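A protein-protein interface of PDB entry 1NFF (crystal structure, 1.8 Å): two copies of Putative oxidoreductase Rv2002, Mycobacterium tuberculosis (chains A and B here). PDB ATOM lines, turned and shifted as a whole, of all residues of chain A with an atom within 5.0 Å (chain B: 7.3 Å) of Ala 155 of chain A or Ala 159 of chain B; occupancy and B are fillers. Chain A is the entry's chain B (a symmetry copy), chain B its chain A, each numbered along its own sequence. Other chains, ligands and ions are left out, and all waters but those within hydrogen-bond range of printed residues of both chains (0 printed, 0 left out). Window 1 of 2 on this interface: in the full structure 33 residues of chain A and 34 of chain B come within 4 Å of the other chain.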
ATOM      1  N   TRP A 105       9.361   2.463 -21.204  1.00  0.00           N
ATOM      2  CA  TRP A 105       9.123   1.160 -20.597  1.00  0.00           C
ATOM      3  C   TRP A 105      10.035   0.965 -19.386  1.00  0.00           C
ATOM      4  O   TRP A 105       9.573   0.594 -18.304  1.00  0.00           O
ATOM      5  CB  TRP A 105       9.352   0.054 -21.639  1.00  0.00           C
ATOM      6  CG  TRP A 105       9.483  -1.345 -21.092  1.00  0.00           C
ATOM      7  CD1 TRP A 105      10.638  -1.970 -20.715  1.00  0.00           C
ATOM      8  CD2 TRP A 105       8.430  -2.299 -20.890  1.00  0.00           C
ATOM      9  NE1 TRP A 105      10.373  -3.253 -20.296  1.00  0.00           N
ATOM     10  CE2 TRP A 105       9.025  -3.482 -20.391  1.00  0.00           C
ATOM     11  CE3 TRP A 105       7.041  -2.271 -21.081  1.00  0.00           C
ATOM     12  CZ2 TRP A 105       8.280  -4.627 -20.080  1.00  0.00           C
ATOM     13  CZ3 TRP A 105       6.299  -3.409 -20.772  1.00  0.00           C
ATOM     14  CH2 TRP A 105       6.921  -4.571 -20.277  1.00  0.00           C
ATOM     15  N   CYS A 150      -1.256   0.362 -23.042  1.00  0.00           N
ATOM     16  CA  CYS A 150      -0.950   0.590 -21.632  1.00  0.00           C
ATOM     17  C   CYS A 150      -0.085  -0.568 -21.123  1.00  0.00           C
ATOM     18  O   CYS A 150      -0.286  -1.082 -20.026  1.00  0.00           O
ATOM     19  CB  CYS A 150      -2.276   0.655 -20.867  1.00  0.00           C
ATOM     20  SG  CYS A 150      -2.181   1.128 -19.143  1.00  0.00           S
ATOM     21  N   HIS A 151       0.901  -0.952 -21.926  1.00  0.00           N
ATOM     22  CA  HIS A 151       1.764  -2.089 -21.622  1.00  0.00           C
ATOM     23  C   HIS A 151       2.700  -1.993 -20.427  1.00  0.00           C
ATOM     24  O   HIS A 151       2.761  -2.919 -19.614  1.00  0.00           O
ATOM     25  CB  HIS A 151       2.526  -2.452 -22.894  1.00  0.00           C
ATOM     26  CG  HIS A 151       1.635  -2.542 -24.091  1.00  0.00           C
ATOM     27  ND1 HIS A 151       0.586  -3.435 -24.164  1.00  0.00           N
ATOM     28  CD2 HIS A 151       1.557  -1.779 -25.207  1.00  0.00           C
ATOM     29  CE1 HIS A 151      -0.100  -3.214 -25.270  1.00  0.00           C
ATOM     30  NE2 HIS A 151       0.467  -2.214 -25.921  1.00  0.00           N
ATOM     31  N   GLY A 152       3.433  -0.891 -20.313  1.00  0.00           N
ATOM     32  CA  GLY A 152       4.333  -0.739 -19.183  1.00  0.00           C
ATOM     33  C   GLY A 152       3.560  -0.568 -17.886  1.00  0.00           C
ATOM     34  O   GLY A 152       3.940  -1.108 -16.850  1.00  0.00           O
ATOM     35  N   TYR A 153       2.463   0.184 -17.946  1.00  0.00           N
ATOM     36  CA  TYR A 153       1.646   0.426 -16.766  1.00  0.00           C
ATOM     37  C   TYR A 153       0.983  -0.874 -16.317  1.00  0.00           C
ATOM     38  O   TYR A 153       0.986  -1.198 -15.134  1.00  0.00           O
ATOM     39  CB  TYR A 153       0.575   1.479 -17.064  1.00  0.00           C
ATOM     40  CG  TYR A 153      -0.130   2.006 -15.837  1.00  0.00           C
ATOM     41  CD1 TYR A 153       0.507   2.892 -14.968  1.00  0.00           C
ATOM     42  CD2 TYR A 153      -1.441   1.631 -15.550  1.00  0.00           C
ATOM     43  CE1 TYR A 153      -0.149   3.398 -13.839  1.00  0.00           C
ATOM     44  CE2 TYR A 153      -2.105   2.125 -14.428  1.00  0.00           C
ATOM     45  CZ  TYR A 153      -1.456   3.007 -13.579  1.00  0.00           C
ATOM     46  OH  TYR A 153      -2.121   3.501 -12.476  1.00  0.00           O
ATOM     47  N   THR A 154       0.414  -1.611 -17.267  1.00  0.00           N
ATOM     48  CA  THR A 154      -0.237  -2.881 -16.961  1.00  0.00           C
ATOM     49  C   THR A 154       0.782  -3.863 -16.380  1.00  0.00           C
ATOM     50  O   THR A 154       0.540  -4.492 -15.351  1.00  0.00           O
ATOM     51  CB  THR A 154      -0.865  -3.508 -18.230  1.00  0.00           C
ATOM     52  OG1 THR A 154      -1.892  -2.645 -18.729  1.00  0.00           O
ATOM     53  CG2 THR A 154      -1.474  -4.871 -17.917  1.00  0.00           C
ATOM     54  N   ALA A 155       1.927  -3.985 -17.044  1.00  0.00           N
ATOM     55  CA  ALA A 155       2.968  -4.893 -16.586  1.00  0.00           C
ATOM     56  C   ALA A 155       3.401  -4.597 -15.150  1.00  0.00           C
ATOM     57  O   ALA A 155       3.489  -5.506 -14.326  1.00  0.00           O
ATOM     58  CB  ALA A 155       4.179  -4.826 -17.524  1.00  0.00           C
ATOM     59  N   THR A 156       3.666  -3.329 -14.846  1.00  0.00           N
ATOM     60  CA  THR A 156       4.102  -2.974 -13.502  1.00  0.00           C
ATOM     61  C   THR A 156       3.008  -3.125 -12.448  1.00  0.00           C
ATOM     62  O   THR A 156       3.284  -3.542 -11.323  1.00  0.00           O
ATOM     63  CB  THR A 156       4.676  -1.532 -13.436  1.00  0.00           C
ATOM     64  OG1 THR A 156       3.693  -0.585 -13.874  1.00  0.00           O
ATOM     65  CG2 THR A 156       5.919  -1.421 -14.314  1.00  0.00           C
ATOM     66  N   LYS A 157       1.768  -2.796 -12.793  1.00  0.00           N
ATOM     67  CA  LYS A 157       0.698  -2.932 -11.811  1.00  0.00           C
ATOM     68  C   LYS A 157       0.418  -4.411 -11.511  1.00  0.00           C
ATOM     69  O   LYS A 157       0.035  -4.753 -10.393  1.00  0.00           O
ATOM     70  CB  LYS A 157      -0.560  -2.198 -12.284  1.00  0.00           C
ATOM     71  CG  LYS A 157      -0.415  -0.667 -12.255  1.00  0.00           C
ATOM     72  CD  LYS A 157       0.063  -0.168 -10.884  1.00  0.00           C
ATOM     73  CE  LYS A 157       0.079   1.360 -10.800  1.00  0.00           C
ATOM     74  NZ  LYS A 157       0.656   1.858  -9.505  1.00  0.00           N
ATOM     75  N   PHE A 158       0.611  -5.282 -12.500  1.00  0.00           N
ATOM     76  CA  PHE A 158       0.433  -6.719 -12.281  1.00  0.00           C
ATOM     77  C   PHE A 158       1.607  -7.197 -11.421  1.00  0.00           C
ATOM     78  O   PHE A 158       1.438  -7.995 -10.499  1.00  0.00           O
ATOM     79  CB  PHE A 158       0.446  -7.495 -13.605  1.00  0.00           C
ATOM     80  CG  PHE A 158      -0.926  -7.860 -14.116  1.00  0.00           C
ATOM     81  CD1 PHE A 158      -1.729  -6.914 -14.752  1.00  0.00           C
ATOM     82  CD2 PHE A 158      -1.416  -9.151 -13.953  1.00  0.00           C
ATOM     83  CE1 PHE A 158      -3.000  -7.252 -15.222  1.00  0.00           C
ATOM     84  CE2 PHE A 158      -2.690  -9.504 -14.419  1.00  0.00           C
ATOM     85  CZ  PHE A 158      -3.483  -8.552 -15.053  1.00  0.00           C
ATOM     86  N   ALA A 159       2.801  -6.702 -11.737  1.00  0.00           N
ATOM     87  CA  ALA A 159       4.002  -7.081 -11.003  1.00  0.00           C
ATOM     88  C   ALA A 159       3.876  -6.714  -9.529  1.00  0.00           C
ATOM     89  O   ALA A 159       4.246  -7.497  -8.658  1.00  0.00           O
ATOM     90  CB  ALA A 159       5.227  -6.402 -11.611  1.00  0.00           C
ATOM     91  N   ASN B 112      13.228 -11.961 -17.917  1.00  0.00           N
ATOM     92  CA  ASN B 112      11.870 -12.483 -17.783  1.00  0.00           C
ATOM     93  C   ASN B 112      10.720 -11.560 -18.168  1.00  0.00           C
ATOM     94  O   ASN B 112       9.655 -12.028 -18.577  1.00  0.00           O
ATOM     95  CB  ASN B 112      11.663 -12.981 -16.350  1.00  0.00           C
ATOM     96  CG  ASN B 112      12.433 -14.259 -16.061  1.00  0.00           C
ATOM     97  OD1 ASN B 112      13.396 -14.582 -16.752  1.00  0.00           O
ATOM     98  ND2 ASN B 112      12.012 -14.989 -15.032  1.00  0.00           N
ATOM     99  N   LEU B 113      10.923 -10.256 -18.040  1.00  0.00           N
ATOM    100  CA  LEU B 113       9.869  -9.309 -18.367  1.00  0.00           C
ATOM    101  C   LEU B 113      10.174  -8.513 -19.626  1.00  0.00           C
ATOM    102  O   LEU B 113       9.457  -8.612 -20.616  1.00  0.00           O
ATOM    103  CB  LEU B 113       9.631  -8.360 -17.186  1.00  0.00           C
ATOM    104  CG  LEU B 113       8.684  -7.182 -17.429  1.00  0.00           C
ATOM    105  CD1 LEU B 113       7.377  -7.670 -18.049  1.00  0.00           C
ATOM    106  CD2 LEU B 113       8.427  -6.465 -16.109  1.00  0.00           C
ATOM    107  N   VAL B 116      10.454 -10.555 -22.795  1.00  0.00           N
ATOM    108  CA  VAL B 116       9.177 -10.980 -23.351  1.00  0.00           C
ATOM    109  C   VAL B 116       8.565  -9.838 -24.153  1.00  0.00           C
ATOM    110  O   VAL B 116       8.040 -10.046 -25.253  1.00  0.00           O
ATOM    111  CB  VAL B 116       8.202 -11.407 -22.225  1.00  0.00           C
ATOM    112  CG1 VAL B 116       6.803 -11.632 -22.785  1.00  0.00           C
ATOM    113  CG2 VAL B 116       8.713 -12.684 -21.567  1.00  0.00           C
ATOM    114  N   PHE B 117       8.637  -8.625 -23.612  1.00  0.00           N
ATOM    115  CA  PHE B 117       8.079  -7.474 -24.311  1.00  0.00           C
ATOM    116  C   PHE B 117       8.833  -7.237 -25.616  1.00  0.00           C
ATOM    117  O   PHE B 117       8.225  -6.942 -26.646  1.00  0.00           O
ATOM    118  CB  PHE B 117       8.134  -6.219 -23.431  1.00  0.00           C
ATOM    119  CG  PHE B 117       7.510  -5.002 -24.066  1.00  0.00           C
ATOM    120  CD1 PHE B 117       6.217  -5.056 -24.586  1.00  0.00           C
ATOM    121  CD2 PHE B 117       8.218  -3.805 -24.155  1.00  0.00           C
ATOM    122  CE1 PHE B 117       5.638  -3.937 -25.189  1.00  0.00           C
ATOM    123  CE2 PHE B 117       7.649  -2.678 -24.755  1.00  0.00           C
ATOM    124  CZ  PHE B 117       6.357  -2.744 -25.275  1.00  0.00           C
ATOM    125  N   SER B 139       4.569 -17.877 -18.633  1.00  0.00           N
ATOM    126  CA  SER B 139       4.526 -17.344 -17.281  1.00  0.00           C
ATOM    127  C   SER B 139       4.696 -18.601 -16.424  1.00  0.00           C
ATOM    128  O   SER B 139       5.499 -19.472 -16.764  1.00  0.00           O
ATOM    129  CB  SER B 139       3.168 -16.680 -17.021  1.00  0.00           C
ATOM    130  OG  SER B 139       3.074 -16.177 -15.698  1.00  0.00           O
ATOM    131  N   GLU B 142       3.778 -19.180 -10.550  1.00  0.00           N
ATOM    132  CA  GLU B 142       4.380 -18.154  -9.701  1.00  0.00           C
ATOM    133  C   GLU B 142       3.908 -16.798 -10.223  1.00  0.00           C
ATOM    134  O   GLU B 142       4.278 -15.747  -9.696  1.00  0.00           O
ATOM    135  CB  GLU B 142       5.915 -18.218  -9.729  1.00  0.00           C
ATOM    136  CG  GLU B 142       6.505 -19.377  -8.932  1.00  0.00           C
ATOM    137  CD  GLU B 142       6.441 -20.696  -9.674  1.00  0.00           C
ATOM    138  OE1 GLU B 142       6.474 -21.753  -9.005  1.00  0.00           O
ATOM    139  OE2 GLU B 142       6.374 -20.677 -10.924  1.00  0.00           O
ATOM    140  N   GLY B 143       3.096 -16.842 -11.278  1.00  0.00           N
ATOM    141  CA  GLY B 143       2.536 -15.630 -11.849  1.00  0.00           C
ATOM    142  C   GLY B 143       1.079 -15.543 -11.424  1.00  0.00           C
ATOM    143  O   GLY B 143       0.345 -14.634 -11.832  1.00  0.00           O
ATOM    144  N   TYR B 153      11.334 -13.316  -9.463  1.00  0.00           N
ATOM    145  CA  TYR B 153      10.670 -14.301 -10.305  1.00  0.00           C
ATOM    146  C   TYR B 153       9.154 -14.133 -10.262  1.00  0.00           C
ATOM    147  O   TYR B 153       8.488 -14.164 -11.298  1.00  0.00           O
ATOM    148  CB  TYR B 153      11.047 -15.711  -9.853  1.00  0.00           C
ATOM    149  CG  TYR B 153      10.677 -16.792 -10.840  1.00  0.00           C
ATOM    150  CD1 TYR B 153      11.387 -16.950 -12.027  1.00  0.00           C
ATOM    151  CD2 TYR B 153       9.634 -17.679 -10.571  1.00  0.00           C
ATOM    152  CE1 TYR B 153      11.074 -17.969 -12.922  1.00  0.00           C
ATOM    153  CE2 TYR B 153       9.313 -18.704 -11.458  1.00  0.00           C
ATOM    154  CZ  TYR B 153      10.036 -18.843 -12.629  1.00  0.00           C
ATOM    155  OH  TYR B 153       9.724 -19.858 -13.507  1.00  0.00           O
ATOM    156  N   THR B 154       8.608 -13.956  -9.063  1.00  0.00           N
ATOM    157  CA  THR B 154       7.167 -13.774  -8.915  1.00  0.00           C
ATOM    158  C   THR B 154       6.728 -12.504  -9.646  1.00  0.00           C
ATOM    159  O   THR B 154       5.793 -12.521 -10.444  1.00  0.00           O
ATOM    160  CB  THR B 154       6.765 -13.658  -7.425  1.00  0.00           C
ATOM    161  OG1 THR B 154       7.030 -14.901  -6.759  1.00  0.00           O
ATOM    162  CG2 THR B 154       5.280 -13.322  -7.297  1.00  0.00           C
ATOM    163  N   ALA B 155       7.423 -11.405  -9.381  1.00  0.00           N
ATOM    164  CA  ALA B 155       7.087 -10.132 -10.010  1.00  0.00           C
ATOM    165  C   ALA B 155       7.087 -10.199 -11.534  1.00  0.00           C
ATOM    166  O   ALA B 155       6.175  -9.677 -12.179  1.00  0.00           O
ATOM    167  CB  ALA B 155       8.053  -9.045  -9.536  1.00  0.00           C
ATOM    168  N   THR B 156       8.100 -10.837 -12.116  1.00  0.00           N
ATOM    169  CA  THR B 156       8.171 -10.919 -13.572  1.00  0.00           C
ATOM    170  C   THR B 156       7.127 -11.852 -14.167  1.00  0.00           C
ATOM    171  O   THR B 156       6.556 -11.561 -15.222  1.00  0.00           O
ATOM    172  CB  THR B 156       9.578 -11.354 -14.067  1.00  0.00           C
ATOM    173  OG1 THR B 156       9.927 -12.621 -13.501  1.00  0.00           O
ATOM    174  CG2 THR B 156      10.623 -10.312 -13.677  1.00  0.00           C
ATOM    175  N   LYS B 157       6.866 -12.973 -13.503  1.00  0.00           N
ATOM    176  CA  LYS B 157       5.876 -13.902 -14.024  1.00  0.00           C
ATOM    177  C   LYS B 157       4.473 -13.301 -13.941  1.00  0.00           C
ATOM    178  O   LYS B 157       3.626 -13.577 -14.794  1.00  0.00           O
ATOM    179  CB  LYS B 157       5.971 -15.241 -13.291  1.00  0.00           C
ATOM    180  CG  LYS B 157       7.262 -15.996 -13.630  1.00  0.00           C
ATOM    181  CD  LYS B 157       7.418 -16.157 -15.147  1.00  0.00           C
ATOM    182  CE  LYS B 157       8.597 -17.057 -15.511  1.00  0.00           C
ATOM    183  NZ  LYS B 157       8.777 -17.183 -16.995  1.00  0.00           N
ATOM    184  N   PHE B 158       4.225 -12.481 -12.921  1.00  0.00           N
ATOM    185  CA  PHE B 158       2.938 -11.801 -12.811  1.00  0.00           C
ATOM    186  C   PHE B 158       2.880 -10.737 -13.905  1.00  0.00           C
ATOM    187  O   PHE B 158       1.836 -10.510 -14.511  1.00  0.00           O
ATOM    188  CB  PHE B 158       2.782 -11.103 -11.459  1.00  0.00           C
ATOM    189  CG  PHE B 158       1.974 -11.879 -10.468  1.00  0.00           C
ATOM    190  CD1 PHE B 158       2.529 -12.959  -9.792  1.00  0.00           C
ATOM    191  CD2 PHE B 158       0.648 -11.528 -10.207  1.00  0.00           C
ATOM    192  CE1 PHE B 158       1.783 -13.682  -8.867  1.00  0.00           C
ATOM    193  CE2 PHE B 158      -0.109 -12.245  -9.282  1.00  0.00           C
ATOM    194  CZ  PHE B 158       0.461 -13.325  -8.610  1.00  0.00           C
ATOM    195  N   ALA B 159       4.008 -10.076 -14.144  1.00  0.00           N
ATOM    196  CA  ALA B 159       4.066  -9.033 -15.164  1.00  0.00           C
ATOM    197  C   ALA B 159       3.792  -9.605 -16.551  1.00  0.00           C
ATOM    198  O   ALA B 159       3.085  -8.992 -17.351  1.00  0.00           O
ATOM    199  CB  ALA B 159       5.431  -8.341 -15.138  1.00  0.00           C
ATOM    200  N   VAL B 160       4.354 -10.777 -16.835  1.00  0.00           N
ATOM    201  CA  VAL B 160       4.152 -11.425 -18.126  1.00  0.00           C
ATOM    202  C   VAL B 160       2.666 -11.746 -18.317  1.00  0.00           C
ATOM    203  O   VAL B 160       2.123 -11.619 -19.416  1.00  0.00           O
ATOM    204  CB  VAL B 160       4.988 -12.731 -18.223  1.00  0.00           C
ATOM    205  CG1 VAL B 160       4.574 -13.535 -19.450  1.00  0.00           C
ATOM    206  CG2 VAL B 160       6.481 -12.385 -18.296  1.00  0.00           C
ATOM    207  N   ARG B 161       2.020 -12.162 -17.235  1.00  0.00           N
ATOM    208  CA  ARG B 161       0.598 -12.482 -17.241  1.00  0.00           C
ATOM    209  C   ARG B 161      -0.205 -11.246 -17.644  1.00  0.00           C
ATOM    210  O   ARG B 161      -1.138 -11.331 -18.443  1.00  0.00           O
ATOM    211  CB  ARG B 161       0.182 -12.936 -15.841  1.00  0.00           C
ATOM    212  CG  ARG B 161      -1.304 -13.168 -15.622  1.00  0.00           C
ATOM    213  CD  ARG B 161      -1.539 -13.423 -14.138  1.00  0.00           C
ATOM    214  NE  ARG B 161      -2.942 -13.606 -13.780  1.00  0.00           N
ATOM    215  CZ  ARG B 161      -3.372 -13.679 -12.524  1.00  0.00           C
ATOM    216  NH1 ARG B 161      -2.502 -13.585 -11.527  1.00  0.00           N
ATOM    217  NH2 ARG B 161      -4.659 -13.852 -12.258  1.00  0.00           N
ATOM    218  N   GLY B 162       0.171 -10.098 -17.085  1.00  0.00           N
ATOM    219  CA  GLY B 162      -0.522  -8.856 -17.396  1.00  0.00           C
ATOM    220  C   GLY B 162      -0.230  -8.325 -18.788  1.00  0.00           C
ATOM    221  O   GLY B 162      -1.138  -7.862 -19.483  1.00  0.00           O
ATOM    222  N   LEU B 163       1.037  -8.381 -19.194  1.00  0.00           N
ATOM    223  CA  LEU B 163       1.444  -7.915 -20.517  1.00  0.00           C
ATOM    224  C   LEU B 163       0.729  -8.732 -21.590  1.00  0.00           C
ATOM    225  O   LEU B 163       0.421  -8.231 -22.671  1.00  0.00           O
ATOM    226  CB  LEU B 163       2.961  -8.061 -20.685  1.00  0.00           C
ATOM    227  CG  LEU B 163       3.568  -7.592 -22.011  1.00  0.00           C
ATOM    228  CD1 LEU B 163       3.381  -6.085 -22.173  1.00  0.00           C
ATOM    229  CD2 LEU B 163       5.054  -7.943 -22.033  1.00  0.00           C
ATOM    230  N   THR B 164       0.468  -9.998 -21.285  1.00  0.00           N
ATOM    231  CA  THR B 164      -0.223 -10.868 -22.223  1.00  0.00           C
ATOM    232  C   THR B 164      -1.593 -10.291 -22.555  1.00  0.00           C
ATOM    233  O   THR B 164      -2.036 -10.330 -23.702  1.00  0.00           O
ATOM    234  CB  THR B 164      -0.405 -12.277 -21.628  1.00  0.00           C
ATOM    235  OG1 THR B 164       0.879 -12.891 -21.476  1.00  0.00           O
ATOM    236  CG2 THR B 164      -1.276 -13.138 -22.529  1.00  0.00           C
ATOM    237  N   LYS B 165      -2.250  -9.739 -21.540  1.00  0.00           N
ATOM    238  CA  LYS B 165      -3.580  -9.168 -21.706  1.00  0.00           C
ATOM    239  C   LYS B 165      -3.584  -7.834 -22.453  1.00  0.00           C
ATOM    240  O   LYS B 165      -4.354  -7.658 -23.399  1.00  0.00           O
ATOM    241  CB  LYS B 165      -4.248  -9.016 -20.335  1.00  0.00           C
ATOM    242  CG  LYS B 165      -4.362 -10.336 -19.568  1.00  0.00           C
ATOM    243  CD  LYS B 165      -4.991 -10.150 -18.190  1.00  0.00           C
ATOM    244  CE  LYS B 165      -4.782 -11.383 -17.314  1.00  0.00           C
ATOM    245  NZ  LYS B 165      -5.286 -12.634 -17.951  1.00  0.00           N
ATOM    246  N   SER B 166      -2.730  -6.900 -22.046  1.00  0.00           N
ATOM    247  CA  SER B 166      -2.695  -5.607 -22.720  1.00  0.00           C
ATOM    248  C   SER B 166      -2.362  -5.765 -24.203  1.00  0.00           C
ATOM    249  O   SER B 166      -3.010  -5.147 -25.054  1.00  0.00           O
ATOM    250  CB  SER B 166      -1.694  -4.648 -22.042  1.00  0.00           C
ATOM    251  OG  SER B 166      -0.359  -5.119 -22.097  1.00  0.00           O
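Among the printed residues, pairs that only touch across the chains: Trp 105 of chain A with Leu 113 of chain B, Trp 105 of chain A with Phe 117 of chain B, His 151 of chain A with Leu 163 of chain B, Thr 154 of chain A with Gly 162 of chain B, Thr 154 of chain A with Ser 166 of chain B, Ala 155 of chain A with Ala 159 of chain B, Phe 158 of chain A with Phe 158 of chain B, Phe 158 of chain A with Gly 162 of chain B, Phe 158 of chain A with Lys 165 of chain B and Ala 159 of chain A with Ala 155 of chain B.
Of the 11 printed residues of chain A, 6 touch a printed residue of chain B. Printed residues of chain A that touch a printed residue of chain B: Trp 105, His 151, Thr 154, Ala 155, Phe 158 and Ala 159. Of the 21 printed residues of chain B, 9 touch a printed residue of chain A. Among the printed residues, no Asp or Glu carboxylate lies within 4 Å of a Lys or Arg side-chain nitrogen of the other chain.
Ala 155 of chain A touches Ala 159 of chain B, and with the chains exchanged Ala 159 of chain A touches Ala 155 of chain B. Phe 158 of chain A touches its own counterpart, Phe 158 of chain B. Positions printed for both chains: 153, 154, 155, 156, 157, 158 and 159. Of the 11 pairs that touch across the chains among the printed residues, 3 have their exchanged pair printed and touching as well.
Ala 155 of chain A touches just one residue of chain B: Ala 159. Of the printed residues of chain A, Gly 162 of chain B touches Thr 154 (3.4 Å) and Phe 158 (3.5 Å). Of the printed residues of chain B, Phe 158 of chain A touches Phe 158 (3.4 Å), Gly 162 (3.5 Å) and Lys 165 (3.8 Å). Of the printed residues of chain A, Phe 158 of chain B touches Phe 158. Of the printed residues of chain A, Leu 163 of chain B touches His 151. The nearest residue of chain B that does not touch Ala 155 of chain A is Leu 113 of chain B (4.3 Å). The nearest residue of chain A that does not touch Ala 159 of chain B is Ala 159 of chain A (4.03 Å).
OG of Ser 166 of chain B lies within hydrogen-bond range of ND1 of His 151 of chain A (2.8 Å).
The backbone carbonyl oxygen of Leu 163 of chain B lies within hydrogen-bond range of the side-chain hydroxyl of Ser 166 of chain B (3.3 Å). The side-chain hydroxyl (OG1) of Thr 154 of chain A is in hydrogen-bond range of the backbone carbonyl oxygen (O) of Cys 150 of chain A, 2.6 Å away.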
